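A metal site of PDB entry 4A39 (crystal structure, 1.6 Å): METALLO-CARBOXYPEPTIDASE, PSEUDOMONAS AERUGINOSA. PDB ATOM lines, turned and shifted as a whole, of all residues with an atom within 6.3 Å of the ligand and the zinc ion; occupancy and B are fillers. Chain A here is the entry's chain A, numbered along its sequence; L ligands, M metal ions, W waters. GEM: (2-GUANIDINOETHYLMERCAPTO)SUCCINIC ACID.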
ATOM      1  N   TYR A  77     -22.731  24.404  28.028  1.00  0.00           N
ATOM      2  CA  TYR A  77     -22.367  24.728  26.655  1.00  0.00           C
ATOM      3  C   TYR A  77     -23.255  25.858  26.155  1.00  0.00           C
ATOM      4  O   TYR A  77     -24.022  25.711  25.205  1.00  0.00           O
ATOM      5  CB  TYR A  77     -22.528  23.473  25.789  1.00  0.00           C
ATOM      6  CG  TYR A  77     -21.832  22.271  26.391  1.00  0.00           C
ATOM      7  CD1 TYR A  77     -20.445  22.225  26.467  1.00  0.00           C
ATOM      8  CD2 TYR A  77     -22.555  21.207  26.922  1.00  0.00           C
ATOM      9  CE1 TYR A  77     -19.785  21.147  27.079  1.00  0.00           C
ATOM     10  CE2 TYR A  77     -21.908  20.127  27.536  1.00  0.00           C
ATOM     11  CZ  TYR A  77     -20.519  20.118  27.610  1.00  0.00           C
ATOM     12  OH  TYR A  77     -19.876  19.063  28.224  1.00  0.00           O
ATOM     13  N   GLN A 179     -23.926   7.670  28.057  1.00  0.00           N
ATOM     14  CA  GLN A 179     -23.121   7.786  29.277  1.00  0.00           C
ATOM     15  C   GLN A 179     -23.471   9.138  29.897  1.00  0.00           C
ATOM     16  O   GLN A 179     -23.435   9.302  31.121  1.00  0.00           O
ATOM     17  CB  GLN A 179     -21.636   7.755  28.965  1.00  0.00           C
ATOM     18  CG  GLN A 179     -21.070   6.389  28.672  1.00  0.00           C
ATOM     19  CD  GLN A 179     -19.564   6.429  28.656  1.00  0.00           C
ATOM     20  OE1 GLN A 179     -18.924   6.448  29.707  1.00  0.00           O
ATOM     21  NE2 GLN A 179     -18.988   6.478  27.459  1.00  0.00           N
ATOM     22  N   HIS A 180     -23.773  10.119  29.045  1.00  0.00           N
ATOM     23  CA  HIS A 180     -24.181  11.445  29.499  1.00  0.00           C
ATOM     24  C   HIS A 180     -25.699  11.420  29.399  1.00  0.00           C
ATOM     25  O   HIS A 180     -26.255  11.370  28.308  1.00  0.00           O
ATOM     26  CB  HIS A 180     -23.552  12.513  28.590  1.00  0.00           C
ATOM     27  CG  HIS A 180     -22.065  12.567  28.699  1.00  0.00           C
ATOM     28  ND1 HIS A 180     -21.238  12.615  27.589  1.00  0.00           N
ATOM     29  CD2 HIS A 180     -21.248  12.577  29.771  1.00  0.00           C
ATOM     30  CE1 HIS A 180     -19.977  12.643  27.989  1.00  0.00           C
ATOM     31  NE2 HIS A 180     -19.956  12.631  29.301  1.00  0.00           N
ATOM     32  N   GLU A 183     -28.125  13.295  26.790  1.00  0.00           N
ATOM     33  CA  GLU A 183     -28.025  13.006  25.360  1.00  0.00           C
ATOM     34  C   GLU A 183     -28.986  11.892  24.941  1.00  0.00           C
ATOM     35  O   GLU A 183     -28.585  10.828  24.469  1.00  0.00           O
ATOM     36  CB  GLU A 183     -26.562  12.666  25.027  1.00  0.00           C
ATOM     37  CG  GLU A 183     -25.667  13.896  25.151  1.00  0.00           C
ATOM     38  CD  GLU A 183     -24.191  13.576  25.305  1.00  0.00           C
ATOM     39  OE1 GLU A 183     -23.749  12.508  24.821  1.00  0.00           O
ATOM     40  OE2 GLU A 183     -23.469  14.401  25.903  1.00  0.00           O
ATOM     41  N   ARG A 231     -24.964  15.789  32.400  1.00  0.00           N
ATOM     42  CA  ARG A 231     -23.626  15.228  32.296  1.00  0.00           C
ATOM     43  C   ARG A 231     -23.139  14.100  33.198  1.00  0.00           C
ATOM     44  O   ARG A 231     -22.425  13.201  32.741  1.00  0.00           O
ATOM     45  CB  ARG A 231     -22.656  16.398  32.441  1.00  0.00           C
ATOM     46  CG  ARG A 231     -21.230  16.114  32.058  1.00  0.00           C
ATOM     47  CD  ARG A 231     -21.081  16.166  30.561  1.00  0.00           C
ATOM     48  NE  ARG A 231     -19.721  15.815  30.167  1.00  0.00           N
ATOM     49  CZ  ARG A 231     -19.334  15.636  28.912  1.00  0.00           C
ATOM     50  NH1 ARG A 231     -20.202  15.770  27.908  1.00  0.00           N
ATOM     51  NH2 ARG A 231     -18.081  15.284  28.662  1.00  0.00           N
ATOM     52  N   ASP A 238     -18.437  12.257  35.727  1.00  0.00           N
ATOM     53  CA  ASP A 238     -18.639  12.281  34.277  1.00  0.00           C
ATOM     54  C   ASP A 238     -18.159  10.892  33.868  1.00  0.00           C
ATOM     55  O   ASP A 238     -16.956  10.621  33.879  1.00  0.00           O
ATOM     56  CB  ASP A 238     -17.748  13.339  33.616  1.00  0.00           C
ATOM     57  CG  ASP A 238     -17.943  13.415  32.104  1.00  0.00           C
ATOM     58  OD1 ASP A 238     -18.335  12.407  31.491  1.00  0.00           O
ATOM     59  OD2 ASP A 238     -17.684  14.496  31.528  1.00  0.00           O
ATOM     60  N   ASN A 240     -17.781   9.494  31.069  1.00  0.00           N
ATOM     61  CA  ASN A 240     -16.840   9.396  29.968  1.00  0.00           C
ATOM     62  C   ASN A 240     -15.474   9.997  30.257  1.00  0.00           C
ATOM     63  O   ASN A 240     -14.721  10.351  29.334  1.00  0.00           O
ATOM     64  CB  ASN A 240     -17.417   9.979  28.687  1.00  0.00           C
ATOM     65  CG  ASN A 240     -16.809   9.326  27.455  1.00  0.00           C
ATOM     66  OD1 ASN A 240     -16.541   8.126  27.465  1.00  0.00           O
ATOM     67  ND2 ASN A 240     -16.603  10.099  26.413  1.00  0.00           N
ATOM     68  N   ARG A 241     -15.141  10.108  31.541  1.00  0.00           N
ATOM     69  CA  ARG A 241     -13.836  10.583  31.986  1.00  0.00           C
ATOM     70  C   ARG A 241     -13.376   9.594  33.060  1.00  0.00           C
ATOM     71  O   ARG A 241     -12.393   9.839  33.757  1.00  0.00           O
ATOM     72  CB  ARG A 241     -13.934  11.985  32.595  1.00  0.00           C
ATOM     73  CG  ARG A 241     -14.295  13.088  31.605  1.00  0.00           C
ATOM     74  CD  ARG A 241     -13.203  13.306  30.576  1.00  0.00           C
ATOM     75  NE  ARG A 241     -13.557  14.401  29.673  1.00  0.00           N
ATOM     76  CZ  ARG A 241     -14.477  14.316  28.713  1.00  0.00           C
ATOM     77  NH1 ARG A 241     -15.129  13.177  28.513  1.00  0.00           N
ATOM     78  NH2 ARG A 241     -14.753  15.374  27.965  1.00  0.00           N
ATOM     79  N   ASP A 271     -19.436   4.325  20.866  1.00  0.00           N
ATOM     80  CA  ASP A 271     -19.948   5.017  22.058  1.00  0.00           C
ATOM     81  C   ASP A 271     -20.884   6.095  21.527  1.00  0.00           C
ATOM     82  O   ASP A 271     -20.450   7.053  20.909  1.00  0.00           O
ATOM     83  CB  ASP A 271     -18.747   5.610  22.816  1.00  0.00           C
ATOM     84  CG  ASP A 271     -19.118   6.215  24.151  1.00  0.00           C
ATOM     85  OD1 ASP A 271     -20.181   5.877  24.703  1.00  0.00           O
ATOM     86  OD2 ASP A 271     -18.313   7.018  24.656  1.00  0.00           O
ATOM     87  N   ILE A 272     -22.189   5.929  21.766  1.00  0.00           N
ATOM     88  CA  ILE A 272     -23.198   6.845  21.243  1.00  0.00           C
ATOM     89  C   ILE A 272     -23.470   8.064  22.127  1.00  0.00           C
ATOM     90  O   ILE A 272     -23.869   7.938  23.284  1.00  0.00           O
ATOM     91  CB  ILE A 272     -24.521   6.106  20.984  1.00  0.00           C
ATOM     92  CG1 ILE A 272     -24.256   4.745  20.320  1.00  0.00           C
ATOM     93  CG2 ILE A 272     -25.414   6.945  20.068  1.00  0.00           C
ATOM     94  CD1 ILE A 272     -23.471   4.825  19.010  1.00  0.00           C
ATOM     95  N   HIS A 273     -23.267   9.244  21.542  1.00  0.00           N
ATOM     96  CA  HIS A 273     -23.414  10.543  22.216  1.00  0.00           C
ATOM     97  C   HIS A 273     -24.214  11.554  21.389  1.00  0.00           C
ATOM     98  O   HIS A 273     -24.666  11.273  20.272  1.00  0.00           O
ATOM     99  CB  HIS A 273     -22.042  11.177  22.473  1.00  0.00           C
ATOM    100  CG  HIS A 273     -21.200  10.454  23.484  1.00  0.00           C
ATOM    101  ND1 HIS A 273     -20.957  10.960  24.741  1.00  0.00           N
ATOM    102  CD2 HIS A 273     -20.499   9.303  23.399  1.00  0.00           C
ATOM    103  CE1 HIS A 273     -20.144  10.146  25.392  1.00  0.00           C
ATOM    104  NE2 HIS A 273     -19.850   9.134  24.593  1.00  0.00           N
ATOM    105  N   GLY A 274     -24.358  12.746  21.952  1.00  0.00           N
ATOM    106  CA  GLY A 274     -25.046  13.842  21.272  1.00  0.00           C
ATOM    107  C   GLY A 274     -24.253  15.113  21.514  1.00  0.00           C
ATOM    108  O   GLY A 274     -23.722  15.304  22.607  1.00  0.00           O
ATOM    109  N   ASP A 275     -24.146  15.960  20.500  1.00  0.00           N
ATOM    110  CA  ASP A 275     -23.410  17.211  20.640  1.00  0.00           C
ATOM    111  C   ASP A 275     -24.361  18.396  20.532  1.00  0.00           C
ATOM    112  O   ASP A 275     -25.124  18.518  19.590  1.00  0.00           O
ATOM    113  CB  ASP A 275     -22.329  17.342  19.559  1.00  0.00           C
ATOM    114  CG  ASP A 275     -21.438  18.555  19.784  1.00  0.00           C
ATOM    115  OD1 ASP A 275     -20.547  18.489  20.664  1.00  0.00           O
ATOM    116  OD2 ASP A 275     -21.642  19.575  19.098  1.00  0.00           O
ATOM    117  N   GLU A 276     -24.284  19.279  21.530  1.00  0.00           N
ATOM    118  CA  GLU A 276     -25.146  20.450  21.614  1.00  0.00           C
ATOM    119  C   GLU A 276     -24.886  21.513  20.548  1.00  0.00           C
ATOM    120  O   GLU A 276     -25.822  22.087  19.986  1.00  0.00           O
ATOM    121  CB  GLU A 276     -24.989  21.097  22.998  1.00  0.00           C
ATOM    122  CG  GLU A 276     -25.403  20.195  24.177  1.00  0.00           C
ATOM    123  CD  GLU A 276     -24.268  19.338  24.726  1.00  0.00           C
ATOM    124  OE1 GLU A 276     -23.265  19.115  24.026  1.00  0.00           O
ATOM    125  OE2 GLU A 276     -24.400  18.855  25.876  1.00  0.00           O
ATOM    126  N   ALA A 284     -16.072  10.742  16.001  1.00  0.00           N
ATOM    127  CA  ALA A 284     -14.733  11.119  16.452  1.00  0.00           C
ATOM    128  C   ALA A 284     -13.942   9.825  16.648  1.00  0.00           C
ATOM    129  O   ALA A 284     -14.374   8.942  17.390  1.00  0.00           O
ATOM    130  CB  ALA A 284     -14.812  11.893  17.759  1.00  0.00           C
ATOM    131  N   GLY A 285     -12.781   9.727  16.001  1.00  0.00           N
ATOM    132  CA  GLY A 285     -11.955   8.528  16.087  1.00  0.00           C
ATOM    133  C   GLY A 285     -10.850   8.508  17.126  1.00  0.00           C
ATOM    134  O   GLY A 285     -10.827   9.328  18.053  1.00  0.00           O
ATOM    135  N   TYR A 319     -15.282  17.259  15.727  1.00  0.00           N
ATOM    136  CA  TYR A 319     -14.248  17.752  16.631  1.00  0.00           C
ATOM    137  C   TYR A 319     -12.900  17.764  15.933  1.00  0.00           C
ATOM    138  O   TYR A 319     -12.672  16.994  14.996  1.00  0.00           O
ATOM    139  CB  TYR A 319     -14.157  16.874  17.887  1.00  0.00           C
ATOM    140  CG  TYR A 319     -15.440  16.738  18.671  1.00  0.00           C
ATOM    141  CD1 TYR A 319     -16.249  17.844  18.914  1.00  0.00           C
ATOM    142  CD2 TYR A 319     -15.835  15.497  19.176  1.00  0.00           C
ATOM    143  CE1 TYR A 319     -17.429  17.727  19.635  1.00  0.00           C
ATOM    144  CE2 TYR A 319     -17.013  15.373  19.908  1.00  0.00           C
ATOM    145  CZ  TYR A 319     -17.810  16.480  20.132  1.00  0.00           C
ATOM    146  OH  TYR A 319     -18.976  16.357  20.845  1.00  0.00           O
ATOM    147  N   PRO A 320     -11.993  18.640  16.367  1.00  0.00           N
ATOM    148  CA  PRO A 320     -10.677  18.695  15.729  1.00  0.00           C
ATOM    149  C   PRO A 320      -9.991  17.355  15.955  1.00  0.00           C
ATOM    150  O   PRO A 320     -10.297  16.653  16.920  1.00  0.00           O
ATOM    151  CB  PRO A 320      -9.968  19.812  16.483  1.00  0.00           C
ATOM    152  CG  PRO A 320     -11.094  20.721  16.888  1.00  0.00           C
ATOM    153  CD  PRO A 320     -12.144  19.723  17.358  1.00  0.00           C
ATOM    154  N   LEU A 331     -11.406   8.812  28.062  1.00  0.00           N
ATOM    155  CA  LEU A 331     -12.627   8.668  27.254  1.00  0.00           C
ATOM    156  C   LEU A 331     -12.770   7.228  26.787  1.00  0.00           C
ATOM    157  O   LEU A 331     -11.785   6.590  26.434  1.00  0.00           O
ATOM    158  CB  LEU A 331     -12.582   9.578  26.029  1.00  0.00           C
ATOM    159  CG  LEU A 331     -12.811  11.080  26.236  1.00  0.00           C
ATOM    160  CD1 LEU A 331     -11.760  11.655  27.180  1.00  0.00           C
ATOM    161  CD2 LEU A 331     -12.750  11.768  24.875  1.00  0.00           C
ATOM    162  N   CYS A 333     -14.035   5.846  24.002  1.00  0.00           N
ATOM    163  CA  CYS A 333     -13.600   5.557  22.640  1.00  0.00           C
ATOM    164  C   CYS A 333     -12.109   5.268  22.580  1.00  0.00           C
ATOM    165  O   CYS A 333     -11.689   4.229  22.068  1.00  0.00           O
ATOM    166  CB  CYS A 333     -13.924   6.738  21.717  1.00  0.00           C
ATOM    167  SG  CYS A 333     -13.423   6.474  20.005  1.00  0.00           S
ATOM    168  N   ASN A 334     -11.313   6.179  23.122  1.00  0.00           N
ATOM    169  CA  ASN A 334      -9.873   6.017  23.121  1.00  0.00           C
ATOM    170  C   ASN A 334      -9.373   4.866  23.988  1.00  0.00           C
ATOM    171  O   ASN A 334      -8.512   4.085  23.556  1.00  0.00           O
ATOM    172  CB  ASN A 334      -9.239   7.327  23.536  1.00  0.00           C
ATOM    173  CG  ASN A 334      -9.489   8.436  22.524  1.00  0.00           C
ATOM    174  OD1 ASN A 334      -8.824   8.498  21.495  1.00  0.00           O
ATOM    175  ND2 ASN A 334     -10.468   9.277  22.800  1.00  0.00           N
ATOM    176  N   THR A 346     -16.699   7.611  18.635  1.00  0.00           N
ATOM    177  CA  THR A 346     -17.665   8.253  19.500  1.00  0.00           C
ATOM    178  C   THR A 346     -18.613   8.749  18.412  1.00  0.00           C
ATOM    179  O   THR A 346     -18.185   9.503  17.537  1.00  0.00           O
ATOM    180  CB  THR A 346     -17.085   9.468  20.243  1.00  0.00           C
ATOM    181  OG1 THR A 346     -16.089   9.035  21.180  1.00  0.00           O
ATOM    182  CG2 THR A 346     -18.184  10.211  20.980  1.00  0.00           C
ATOM    183  N   ILE A 347     -19.868   8.304  18.419  1.00  0.00           N
ATOM    184  CA  ILE A 347     -20.824   8.745  17.418  1.00  0.00           C
ATOM    185  C   ILE A 347     -21.557   9.943  18.002  1.00  0.00           C
ATOM    186  O   ILE A 347     -22.027   9.897  19.141  1.00  0.00           O
ATOM    187  CB  ILE A 347     -21.856   7.628  17.056  1.00  0.00           C
ATOM    188  CG1 ILE A 347     -21.132   6.416  16.457  1.00  0.00           C
ATOM    189  CG2 ILE A 347     -22.893   8.166  16.084  1.00  0.00           C
ATOM    190  CD1 ILE A 347     -20.400   6.721  15.166  1.00  0.00           C
ATOM    191  N   GLU A 348     -21.651  11.023  17.226  1.00  0.00           N
ATOM    192  CA  GLU A 348     -22.282  12.242  17.688  1.00  0.00           C
ATOM    193  C   GLU A 348     -23.464  12.708  16.841  1.00  0.00           C
ATOM    194  O   GLU A 348     -23.311  12.986  15.658  1.00  0.00           O
ATOM    195  CB  GLU A 348     -21.248  13.369  17.740  1.00  0.00           C
ATOM    196  CG  GLU A 348     -20.095  13.150  18.700  1.00  0.00           C
ATOM    197  CD  GLU A 348     -20.474  13.326  20.148  1.00  0.00           C
ATOM    198  OE1 GLU A 348     -21.572  13.855  20.424  1.00  0.00           O
ATOM    199  OE2 GLU A 348     -19.671  12.927  21.023  1.00  0.00           O
HETATM  200  C8  GEM L   1     -17.304  13.783  24.174  1.00  0.00           C
HETATM  201  S7  GEM L   1     -17.546  12.059  23.626  1.00  0.00           S
HETATM  202  C6  GEM L   1     -16.090  11.844  22.545  1.00  0.00           C
HETATM  203  C5  GEM L   1     -15.605  13.127  21.866  1.00  0.00           C
HETATM  204  N3  GEM L   1     -14.976  14.020  22.854  1.00  0.00           N
HETATM  205  C1  GEM L   1     -13.678  14.289  22.751  1.00  0.00           C
HETATM  206  N4  GEM L   1     -12.964  13.738  21.772  1.00  0.00           N
HETATM  207  N2  GEM L   1     -13.085  15.099  23.625  1.00  0.00           N
HETATM  208  C9  GEM L   1     -17.201  13.884  25.702  1.00  0.00           C
HETATM  209  O14 GEM L   1     -17.184  12.814  26.348  1.00  0.00           O
HETATM  210  O15 GEM L   1     -17.142  15.030  26.180  1.00  0.00           O
HETATM  211  C10 GEM L   1     -18.427  14.684  23.650  1.00  0.00           C
HETATM  212  C11 GEM L   1     -19.799  14.264  24.188  1.00  0.00           C
HETATM  213  O12 GEM L   1     -20.711  14.089  23.348  1.00  0.00           O
HETATM  214  O13 GEM L   1     -19.906  14.142  25.425  1.00  0.00           O
HETATM  215 ZN    ZN M   1     -21.688  12.821  25.551  1.00  0.00          ZN
HETATM  216  O   HOH W   1     -22.127  16.670  24.416  1.00  0.00           O
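The backbone carbonyl oxygen (O) of Gly 274 sits close to an oxygen (O12) of the ligand.
Merely in contact with the ligand: Tyr 319, Leu 331 and Thr 346.
Hydrophobic or aromatic side chains that line the ligand: His 180, His 273, Tyr 319 and Leu 331.
11 residues have an atom within 4 Å of the ligand: His 180, Glu 183, Arg 231, Asn 240, Arg 241, His 273, Gly 274, Tyr 319, Leu 331, Thr 346 and Glu 348.
NE2 of His 180 sits close to NE of Arg 231, 3.3 Å away.
A ring nitrogen (NE2) of His 180 sits at hydrogen-bond distance from the side-chain carboxylate (OD1) of Asp 238, 2.7 Å away.
OD2 of Asp 271 is in hydrogen-bond range of NE2 of His 273 (2.6 Å).
The side-chain carboxylate of Asp 275 is in hydrogen-bond range of the side-chain hydroxyl of Tyr 319 (2.7 Å).
The guanidinium group (NH1) of Arg 231 sits at hydrogen-bond distance from the side-chain hydroxyl (OH) of Tyr 77.
The side-chain sulfur (SG) of Cys 333 is in hydrogen-bond range of the backbone NH (N) of Thr 346 (3.7 Å).
The backbone NH of His 273 lies within hydrogen-bond range of the backbone carbonyl oxygen of Ile 347 (2.8 Å).
The side-chain amide oxygen of Asn 240 lies within hydrogen-bond range of the side-chain amide nitrogen of Gln 179 (3.0 Å).
The zinc ion is bound by a ring nitrogen (ND1) of His 180 (2.1 Å).
The zinc ion is bound by ND1 of His 273.
OE1 of Glu 183 binds the zinc ion (2.2 Å).
An oxygen (O13) of the ligand is bound to the zinc ion.
The side-chain carboxylate (OE2) of Glu 183 binds the zinc ion.
Slightly farther from the zinc ion lies an oxygen (O12) of the ligand (2.7 Å).
The guanidinium group of Arg 231 is in salt-bridge range of an oxygen (O15) of the ligand.
ND2 of Asn 240 sits at hydrogen-bond distance from O14 of the ligand.
The side-chain carboxylate (OE2) of Glu 348 lies close to an oxygen (O12) of the ligand.
The guanidinium group (NH2) of Arg 241 is in salt-bridge range of an oxygen (O15) of the ligand (3.0 Å).
Water W1 lies within hydrogen-bond range of the side-chain carboxylate (OE1) of Glu 276, the backbone carbonyl oxygen (O) of Gly 274 and an oxygen (O12) of the ligand.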
